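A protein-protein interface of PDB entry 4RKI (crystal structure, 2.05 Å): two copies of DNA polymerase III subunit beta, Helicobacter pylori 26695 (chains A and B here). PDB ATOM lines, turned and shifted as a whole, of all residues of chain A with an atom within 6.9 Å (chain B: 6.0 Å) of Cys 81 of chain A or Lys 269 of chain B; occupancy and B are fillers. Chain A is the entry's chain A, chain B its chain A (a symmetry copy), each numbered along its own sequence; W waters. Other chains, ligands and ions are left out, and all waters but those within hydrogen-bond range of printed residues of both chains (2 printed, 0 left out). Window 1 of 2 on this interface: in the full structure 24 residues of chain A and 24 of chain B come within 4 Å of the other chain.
OE2 of Glu 266 of chain B lies within salt-bridge range of NZ of Lys 83 of chain A.
O of Lys 269 of chain B sits at hydrogen-bond distance from SG of Cys 81 of chain A, at 3.7 Å.
NE2 of Gln 100 of chain A sits at hydrogen-bond distance from O of Lys 83 of chain A.
SG of Cys 81 of chain A lies within hydrogen-bond range of O of Asp 77 of chain A, 3.5 Å away.
The backbone carbonyl oxygen of Leu 270 of chain B is in hydrogen-bond range of the side-chain hydroxyl of Ser 273 of chain B (2.6 Å).
O of Lys 269 of chain B sits at hydrogen-bond distance from OG of Ser 272 of chain B (3.2 Å).
Among the printed residues, merely in contact across the chains: Ile 78 of chain A with Ser 273 of chain B (3.6 Å), Cys 81 of chain A with Leu 270 of chain B (3.9 Å), Leu 82 of chain A with Leu 270 of chain B (3.8 Å), Ser 103 of chain A with Leu 270 of chain B (3.4 Å) and Phe 105 of chain A with Leu 270 of chain B (3.4 Å).
Of chain B, only Lys 269 (3.7 Å) and Leu 270 (3.9 Å) come within 4 Å of Cys 81 of chain A.
Printed residues of chain B within 4 Å of Ser 103 of chain A: Leu 270.
Ser 267 of chain B touches none of the printed residues of chain A.
Lys 269 of chain B touches one residue of chain A.
Of the printed residues of chain A, Ser 273 of chain B touches Ile 78 (3.6 Å).
The nearest residue of chain A that does not touch Lys 269 of chain B is Asp 77 of chain A (6.3 Å).
The nearest printed residue of chain A that does not touch Leu 270 of chain B is Ile 78 of chain A (5.7 Å).
Of the 13 printed residues of chain A, 6 touch a printed residue of chain B.
Hydrophobic or aromatic side chains of chain A that line the printed part of chain B: Ile 78, Leu 82 and Phe 105.
Hydrophobic or aromatic side chains of chain B within 4 Å of the printed part of chain A: Leu 270.
Along chain B the printed residues that touch a printed residue of chain A span positions 266 to 273.
Among the printed residues, 7 pairs touch across the chains.
Among the printed residues, Asp or Glu carboxylates within 4 Å of a Lys or Arg side-chain nitrogen of the other chain: Lys 83 of chain A with Glu 266 of chain B (3.0 Å).
No position is printed for both chains.
Of the 7 pairs that touch across the chains among the printed residues, none has its exchanged pair printed and touching as well.
Water W1 lies within hydrogen-bond range of the side-chain carboxylate of Asp 77 of chain A (2.6 Å) and the backbone carbonyl oxygen of Ser 273 of chain B (2.7 Å).
Water W2 lies within hydrogen-bond range of the backbone carbonyl oxygen of Glu 266 of chain B (2.8 Å) and the backbone carbonyl oxygen of Cys 81 of chain A (3.0 Å).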
ATOM      1  N   LYS A   7      -5.660 -15.729  33.827  1.00  0.00           N
ATOM      2  CA  LYS A   7      -5.424 -14.347  33.417  1.00  0.00           C
ATOM      3  C   LYS A   7      -5.986 -13.364  34.435  1.00  0.00           C
ATOM      4  O   LYS A   7      -5.280 -12.465  34.873  1.00  0.00           O
ATOM      5  CB  LYS A   7      -6.001 -14.104  32.018  1.00  0.00           C
ATOM      6  CG  LYS A   7      -5.736 -12.715  31.443  1.00  0.00           C
ATOM      7  CD  LYS A   7      -6.882 -11.753  31.714  1.00  0.00           C
ATOM      8  CE  LYS A   7      -6.705 -10.468  30.930  1.00  0.00           C
ATOM      9  NZ  LYS A   7      -7.982  -9.723  30.811  1.00  0.00           N
ATOM     10  N   GLU A  11      -3.854 -10.743  36.623  1.00  0.00           N
ATOM     11  CA  GLU A  11      -4.126  -9.316  36.423  1.00  0.00           C
ATOM     12  C   GLU A  11      -4.445  -8.617  37.735  1.00  0.00           C
ATOM     13  O   GLU A  11      -3.853  -7.597  38.060  1.00  0.00           O
ATOM     14  CB  GLU A  11      -5.287  -9.125  35.453  1.00  0.00           C
ATOM     15  CG  GLU A  11      -5.549  -7.661  35.110  1.00  0.00           C
ATOM     16  CD  GLU A  11      -6.402  -7.475  33.872  1.00  0.00           C
ATOM     17  OE1 GLU A  11      -7.019  -8.462  33.415  1.00  0.00           O
ATOM     18  OE2 GLU A  11      -6.459  -6.334  33.361  1.00  0.00           O
ATOM     19  N   LEU A  76       1.864  -5.857  33.772  1.00  0.00           N
ATOM     20  CA  LEU A  76       0.438  -5.574  33.860  1.00  0.00           C
ATOM     21  C   LEU A  76      -0.121  -5.062  32.528  1.00  0.00           C
ATOM     22  O   LEU A  76      -1.210  -5.472  32.121  1.00  0.00           O
ATOM     23  CB  LEU A  76       0.153  -4.563  34.968  1.00  0.00           C
ATOM     24  CG  LEU A  76      -1.276  -4.020  35.041  1.00  0.00           C
ATOM     25  CD1 LEU A  76      -2.308  -5.119  35.218  1.00  0.00           C
ATOM     26  CD2 LEU A  76      -1.385  -3.012  36.164  1.00  0.00           C
ATOM     27  N   ASP A  77       0.603  -4.167  31.859  1.00  0.00           N
ATOM     28  CA  ASP A  77       0.144  -3.660  30.564  1.00  0.00           C
ATOM     29  C   ASP A  77      -0.052  -4.816  29.584  1.00  0.00           C
ATOM     30  O   ASP A  77      -1.043  -4.853  28.852  1.00  0.00           O
ATOM     31  CB  ASP A  77       1.126  -2.653  29.970  1.00  0.00           C
ATOM     32  CG  ASP A  77       1.147  -1.327  30.722  1.00  0.00           C
ATOM     33  OD1 ASP A  77       0.217  -1.042  31.498  1.00  0.00           O
ATOM     34  OD2 ASP A  77       2.125  -0.573  30.538  1.00  0.00           O
ATOM     35  N   ILE A  78       0.879  -5.770  29.587  1.00  0.00           N
ATOM     36  CA  ILE A  78       0.767  -6.920  28.692  1.00  0.00           C
ATOM     37  C   ILE A  78      -0.460  -7.772  28.999  1.00  0.00           C
ATOM     38  O   ILE A  78      -1.264  -8.053  28.107  1.00  0.00           O
ATOM     39  CB  ILE A  78       2.024  -7.800  28.733  1.00  0.00           C
ATOM     40  CG1 ILE A  78       3.185  -7.069  28.067  1.00  0.00           C
ATOM     41  CG2 ILE A  78       1.775  -9.124  28.021  1.00  0.00           C
ATOM     42  CD1 ILE A  78       4.531  -7.719  28.299  1.00  0.00           C
ATOM     43  N   ILE A  79      -0.602  -8.166  30.258  1.00  0.00           N
ATOM     44  CA  ILE A  79      -1.668  -9.064  30.686  1.00  0.00           C
ATOM     45  C   ILE A  79      -3.048  -8.458  30.444  1.00  0.00           C
ATOM     46  O   ILE A  79      -3.958  -9.141  29.986  1.00  0.00           O
ATOM     47  CB  ILE A  79      -1.533  -9.431  32.193  1.00  0.00           C
ATOM     48  CG1 ILE A  79      -0.217 -10.172  32.473  1.00  0.00           C
ATOM     49  CG2 ILE A  79      -2.705 -10.284  32.663  1.00  0.00           C
ATOM     50  CD1 ILE A  79       0.114 -11.269  31.485  1.00  0.00           C
ATOM     51  N   SER A  80      -3.207  -7.173  30.732  1.00  0.00           N
ATOM     52  CA  SER A  80      -4.504  -6.534  30.554  1.00  0.00           C
ATOM     53  C   SER A  80      -4.925  -6.484  29.067  1.00  0.00           C
ATOM     54  O   SER A  80      -6.095  -6.258  28.765  1.00  0.00           O
ATOM     55  CB  SER A  80      -4.492  -5.141  31.184  1.00  0.00           C
ATOM     56  OG  SER A  80      -3.545  -4.310  30.536  1.00  0.00           O
ATOM     57  N   CYS A  81      -3.980  -6.710  28.155  1.00  0.00           N
ATOM     58  CA  CYS A  81      -4.273  -6.764  26.719  1.00  0.00           C
ATOM     59  C   CYS A  81      -4.621  -8.164  26.207  1.00  0.00           C
ATOM     60  O   CYS A  81      -4.920  -8.332  25.029  1.00  0.00           O
ATOM     61  CB  CYS A  81      -3.084  -6.228  25.911  1.00  0.00           C
ATOM     62  SG  CYS A  81      -2.954  -4.434  25.911  1.00  0.00           S
ATOM     63  N   LEU A  82      -4.585  -9.163  27.077  1.00  0.00           N
ATOM     64  CA  LEU A  82      -4.810 -10.534  26.654  1.00  0.00           C
ATOM     65  C   LEU A  82      -6.261 -10.953  26.816  1.00  0.00           C
ATOM     66  O   LEU A  82      -7.053 -10.280  27.479  1.00  0.00           O
ATOM     67  CB  LEU A  82      -3.896 -11.478  27.442  1.00  0.00           C
ATOM     68  CG  LEU A  82      -2.419 -11.323  27.085  1.00  0.00           C
ATOM     69  CD1 LEU A  82      -1.556 -12.240  27.939  1.00  0.00           C
ATOM     70  CD2 LEU A  82      -2.194 -11.605  25.608  1.00  0.00           C
ATOM     71  N   LYS A  83      -6.587 -12.087  26.204  1.00  0.00           N
ATOM     72  CA  LYS A  83      -7.895 -12.715  26.345  1.00  0.00           C
ATOM     73  C   LYS A  83      -7.960 -13.377  27.712  1.00  0.00           C
ATOM     74  O   LYS A  83      -6.962 -13.428  28.423  1.00  0.00           O
ATOM     75  CB  LYS A  83      -8.104 -13.755  25.243  1.00  0.00           C
ATOM     76  CG  LYS A  83      -8.024 -13.191  23.826  1.00  0.00           C
ATOM     77  CD  LYS A  83      -7.820 -14.297  22.800  1.00  0.00           C
ATOM     78  CE  LYS A  83      -7.521 -13.739  21.413  1.00  0.00           C
ATOM     79  NZ  LYS A  83      -8.607 -12.858  20.894  1.00  0.00           N
ATOM     80  N   GLN A 100       0.108 -16.816  25.406  1.00  0.00           N
ATOM     81  CA  GLN A 100      -1.296 -17.153  25.411  1.00  0.00           C
ATOM     82  C   GLN A 100      -1.662 -17.386  23.958  1.00  0.00           C
ATOM     83  O   GLN A 100      -1.809 -16.430  23.188  1.00  0.00           O
ATOM     84  CB  GLN A 100      -2.124 -16.014  25.990  1.00  0.00           C
ATOM     85  CG  GLN A 100      -3.593 -16.362  26.155  1.00  0.00           C
ATOM     86  CD  GLN A 100      -4.469 -15.144  26.348  1.00  0.00           C
ATOM     87  OE1 GLN A 100      -4.572 -14.287  25.463  1.00  0.00           O
ATOM     88  NE2 GLN A 100      -5.122 -15.068  27.499  1.00  0.00           N
ATOM     89  N   SER A 103      -0.340 -15.331  20.975  1.00  0.00           N
ATOM     90  CA  SER A 103       0.344 -14.155  21.504  1.00  0.00           C
ATOM     91  C   SER A 103       1.519 -14.558  22.381  1.00  0.00           C
ATOM     92  O   SER A 103       1.369 -15.407  23.259  1.00  0.00           O
ATOM     93  CB  SER A 103      -0.632 -13.316  22.313  1.00  0.00           C
ATOM     94  OG  SER A 103      -1.687 -12.854  21.486  1.00  0.00           O
ATOM     95  N   PHE A 105       5.296 -12.935  24.441  1.00  0.00           N
ATOM     96  CA  PHE A 105       6.056 -11.770  24.888  1.00  0.00           C
ATOM     97  C   PHE A 105       7.324 -12.178  25.607  1.00  0.00           C
ATOM     98  O   PHE A 105       7.398 -13.266  26.191  1.00  0.00           O
ATOM     99  CB  PHE A 105       5.226 -10.916  25.848  1.00  0.00           C
ATOM    100  CG  PHE A 105       3.836 -10.622  25.363  1.00  0.00           C
ATOM    101  CD1 PHE A 105       2.844 -11.588  25.442  1.00  0.00           C
ATOM    102  CD2 PHE A 105       3.516  -9.375  24.845  1.00  0.00           C
ATOM    103  CE1 PHE A 105       1.568 -11.330  24.996  1.00  0.00           C
ATOM    104  CE2 PHE A 105       2.235  -9.105  24.401  1.00  0.00           C
ATOM    105  CZ  PHE A 105       1.258 -10.086  24.478  1.00  0.00           C
ATOM    106  N   GLU B 262     -11.780  -5.260  14.310  1.00  0.00           N
ATOM    107  CA  GLU B 262     -11.634  -5.462  15.759  1.00  0.00           C
ATOM    108  C   GLU B 262     -10.459  -6.379  16.075  1.00  0.00           C
ATOM    109  O   GLU B 262      -9.754  -6.175  17.066  1.00  0.00           O
ATOM    110  CB  GLU B 262     -12.915  -6.013  16.385  1.00  0.00           C
ATOM    111  CG  GLU B 262     -14.083  -5.038  16.419  1.00  0.00           C
ATOM    112  CD  GLU B 262     -13.771  -3.728  17.120  1.00  0.00           C
ATOM    113  OE1 GLU B 262     -13.123  -3.757  18.175  1.00  0.00           O
ATOM    114  OE2 GLU B 262     -14.171  -2.653  16.610  1.00  0.00           O
ATOM    115  N   PHE B 264      -7.737  -6.527  14.292  1.00  0.00           N
ATOM    116  CA  PHE B 264      -6.575  -5.654  14.121  1.00  0.00           C
ATOM    117  C   PHE B 264      -6.396  -4.652  15.288  1.00  0.00           C
ATOM    118  O   PHE B 264      -5.282  -4.386  15.708  1.00  0.00           O
ATOM    119  CB  PHE B 264      -6.624  -4.929  12.765  1.00  0.00           C
ATOM    120  CG  PHE B 264      -5.895  -5.673  11.673  1.00  0.00           C
ATOM    121  CD1 PHE B 264      -6.352  -6.903  11.238  1.00  0.00           C
ATOM    122  CD2 PHE B 264      -4.732  -5.160  11.116  1.00  0.00           C
ATOM    123  CE1 PHE B 264      -5.661  -7.616  10.264  1.00  0.00           C
ATOM    124  CE2 PHE B 264      -4.044  -5.860  10.137  1.00  0.00           C
ATOM    125  CZ  PHE B 264      -4.507  -7.095   9.714  1.00  0.00           C
ATOM    126  N   LYS B 265      -7.487  -4.101  15.797  1.00  0.00           N
ATOM    127  CA  LYS B 265      -7.418  -3.219  16.963  1.00  0.00           C
ATOM    128  C   LYS B 265      -6.818  -3.939  18.173  1.00  0.00           C
ATOM    129  O   LYS B 265      -5.903  -3.441  18.827  1.00  0.00           O
ATOM    130  CB  LYS B 265      -8.813  -2.745  17.350  1.00  0.00           C
ATOM    131  CG  LYS B 265      -9.380  -1.626  16.500  1.00  0.00           C
ATOM    132  CD  LYS B 265     -10.654  -1.117  17.171  1.00  0.00           C
ATOM    133  CE  LYS B 265     -11.456  -0.189  16.289  1.00  0.00           C
ATOM    134  NZ  LYS B 265     -12.724   0.244  16.951  1.00  0.00           N
ATOM    135  N   GLU B 266      -7.363  -5.111  18.456  1.00  0.00           N
ATOM    136  CA  GLU B 266      -6.927  -5.932  19.569  1.00  0.00           C
ATOM    137  C   GLU B 266      -5.436  -6.290  19.426  1.00  0.00           C
ATOM    138  O   GLU B 266      -4.652  -6.143  20.364  1.00  0.00           O
ATOM    139  CB  GLU B 266      -7.798  -7.188  19.608  1.00  0.00           C
ATOM    140  CG  GLU B 266      -7.807  -7.935  20.919  1.00  0.00           C
ATOM    141  CD  GLU B 266      -8.608  -9.225  20.843  1.00  0.00           C
ATOM    142  OE1 GLU B 266      -9.223  -9.496  19.783  1.00  0.00           O
ATOM    143  OE2 GLU B 266      -8.620  -9.969  21.850  1.00  0.00           O
ATOM    144  N   SER B 267      -5.042  -6.727  18.237  1.00  0.00           N
ATOM    145  CA  SER B 267      -3.657  -7.127  17.998  1.00  0.00           C
ATOM    146  C   SER B 267      -2.680  -5.956  18.075  1.00  0.00           C
ATOM    147  O   SER B 267      -1.567  -6.102  18.594  1.00  0.00           O
ATOM    148  CB  SER B 267      -3.542  -7.831  16.655  1.00  0.00           C
ATOM    149  OG  SER B 267      -4.526  -8.841  16.582  1.00  0.00           O
ATOM    150  N   ILE B 268      -3.095  -4.790  17.588  1.00  0.00           N
ATOM    151  CA  ILE B 268      -2.241  -3.606  17.639  1.00  0.00           C
ATOM    152  C   ILE B 268      -2.103  -3.061  19.071  1.00  0.00           C
ATOM    153  O   ILE B 268      -0.995  -2.736  19.503  1.00  0.00           O
ATOM    154  CB  ILE B 268      -2.745  -2.515  16.677  1.00  0.00           C
ATOM    155  CG1 ILE B 268      -2.465  -2.945  15.232  1.00  0.00           C
ATOM    156  CG2 ILE B 268      -2.081  -1.185  16.980  1.00  0.00           C
ATOM    157  CD1 ILE B 268      -3.310  -2.243  14.192  1.00  0.00           C
ATOM    158  N   LYS B 269      -3.217  -2.949  19.786  1.00  0.00           N
ATOM    159  CA  LYS B 269      -3.180  -2.573  21.211  1.00  0.00           C
ATOM    160  C   LYS B 269      -2.258  -3.493  21.995  1.00  0.00           C
ATOM    161  O   LYS B 269      -1.461  -3.045  22.806  1.00  0.00           O
ATOM    162  CB  LYS B 269      -4.578  -2.621  21.828  1.00  0.00           C
ATOM    163  CG  LYS B 269      -5.437  -1.438  21.428  1.00  0.00           C
ATOM    164  CD  LYS B 269      -6.900  -1.627  21.792  1.00  0.00           C
ATOM    165  CE  LYS B 269      -7.730  -0.497  21.199  1.00  0.00           C
ATOM    166  NZ  LYS B 269      -9.199  -0.669  21.403  1.00  0.00           N
ATOM    167  N   LEU B 270      -2.370  -4.785  21.731  1.00  0.00           N
ATOM    168  CA  LEU B 270      -1.546  -5.780  22.395  1.00  0.00           C
ATOM    169  C   LEU B 270      -0.051  -5.507  22.219  1.00  0.00           C
ATOM    170  O   LEU B 270       0.687  -5.481  23.209  1.00  0.00           O
ATOM    171  CB  LEU B 270      -1.923  -7.171  21.881  1.00  0.00           C
ATOM    172  CG  LEU B 270      -1.150  -8.377  22.404  1.00  0.00           C
ATOM    173  CD1 LEU B 270      -2.047  -9.600  22.366  1.00  0.00           C
ATOM    174  CD2 LEU B 270       0.133  -8.619  21.619  1.00  0.00           C
ATOM    175  N   CYS B 271       0.400  -5.310  20.974  1.00  0.00           N
ATOM    176  CA  CYS B 271       1.823  -5.051  20.704  1.00  0.00           C
ATOM    177  C   CYS B 271       2.275  -3.683  21.209  1.00  0.00           C
ATOM    178  O   CYS B 271       3.437  -3.514  21.575  1.00  0.00           O
ATOM    179  CB  CYS B 271       2.158  -5.183  19.216  1.00  0.00           C
ATOM    180  SG  CYS B 271       1.967  -6.855  18.565  1.00  0.00           S
ATOM    181  N   SER B 272       1.367  -2.712  21.257  1.00  0.00           N
ATOM    182  CA  SER B 272       1.735  -1.385  21.746  1.00  0.00           C
ATOM    183  C   SER B 272       1.875  -1.334  23.266  1.00  0.00           C
ATOM    184  O   SER B 272       2.175  -0.283  23.822  1.00  0.00           O
ATOM    185  CB  SER B 272       0.789  -0.278  21.234  1.00  0.00           C
ATOM    186  OG  SER B 272      -0.438  -0.772  20.748  1.00  0.00           O
ATOM    187  N   SER B 273       1.679  -2.463  23.945  1.00  0.00           N
ATOM    188  CA  SER B 273       2.018  -2.528  25.352  1.00  0.00           C
ATOM    189  C   SER B 273       3.519  -2.302  25.540  1.00  0.00           C
ATOM    190  O   SER B 273       3.931  -1.804  26.580  1.00  0.00           O
ATOM    191  CB  SER B 273       1.567  -3.851  25.974  1.00  0.00           C
ATOM    192  OG  SER B 273       2.166  -4.955  25.332  1.00  0.00           O
ATOM    193  N   ILE B 278       4.830  -0.875  15.101  1.00  0.00           N
ATOM    194  CA  ILE B 278       4.579  -2.291  14.914  1.00  0.00           C
ATOM    195  C   ILE B 278       4.987  -2.717  13.508  1.00  0.00           C
ATOM    196  O   ILE B 278       4.816  -1.959  12.540  1.00  0.00           O
ATOM    197  CB  ILE B 278       3.083  -2.594  15.129  1.00  0.00           C
ATOM    198  CG1 ILE B 278       2.708  -2.330  16.590  1.00  0.00           C
ATOM    199  CG2 ILE B 278       2.744  -4.032  14.742  1.00  0.00           C
ATOM    200  CD1 ILE B 278       1.236  -2.454  16.876  1.00  0.00           C
ATOM    201  N   LEU B 326      -4.582   2.644  14.883  1.00  0.00           N
ATOM    202  CA  LEU B 326      -5.755   2.441  15.732  1.00  0.00           C
ATOM    203  C   LEU B 326      -6.792   3.539  15.530  1.00  0.00           C
ATOM    204  O   LEU B 326      -7.986   3.264  15.406  1.00  0.00           O
ATOM    205  CB  LEU B 326      -5.351   2.382  17.211  1.00  0.00           C
ATOM    206  CG  LEU B 326      -4.733   1.077  17.681  1.00  0.00           C
ATOM    207  CD1 LEU B 326      -4.268   1.189  19.137  1.00  0.00           C
ATOM    208  CD2 LEU B 326      -5.729  -0.061  17.515  1.00  0.00           C
ATOM    209  N   ASN B 330     -10.566   3.304  14.477  1.00  0.00           N
ATOM    210  CA  ASN B 330     -11.589   3.939  15.314  1.00  0.00           C
ATOM    211  C   ASN B 330     -12.574   4.810  14.540  1.00  0.00           C
ATOM    212  O   ASN B 330     -13.739   4.907  14.919  1.00  0.00           O
ATOM    213  CB  ASN B 330     -10.939   4.771  16.424  1.00  0.00           C
ATOM    214  CG  ASN B 330     -10.287   3.918  17.487  1.00  0.00           C
ATOM    215  OD1 ASN B 330     -10.564   2.724  17.608  1.00  0.00           O
ATOM    216  ND2 ASN B 330      -9.399   4.530  18.266  1.00  0.00           N
HETATM  217  O   HOH W   1       4.270  -1.241  29.189  1.00  0.00           O
HETATM  218  O   HOH W   2      -5.486  -6.162  23.058  1.00  0.00           O
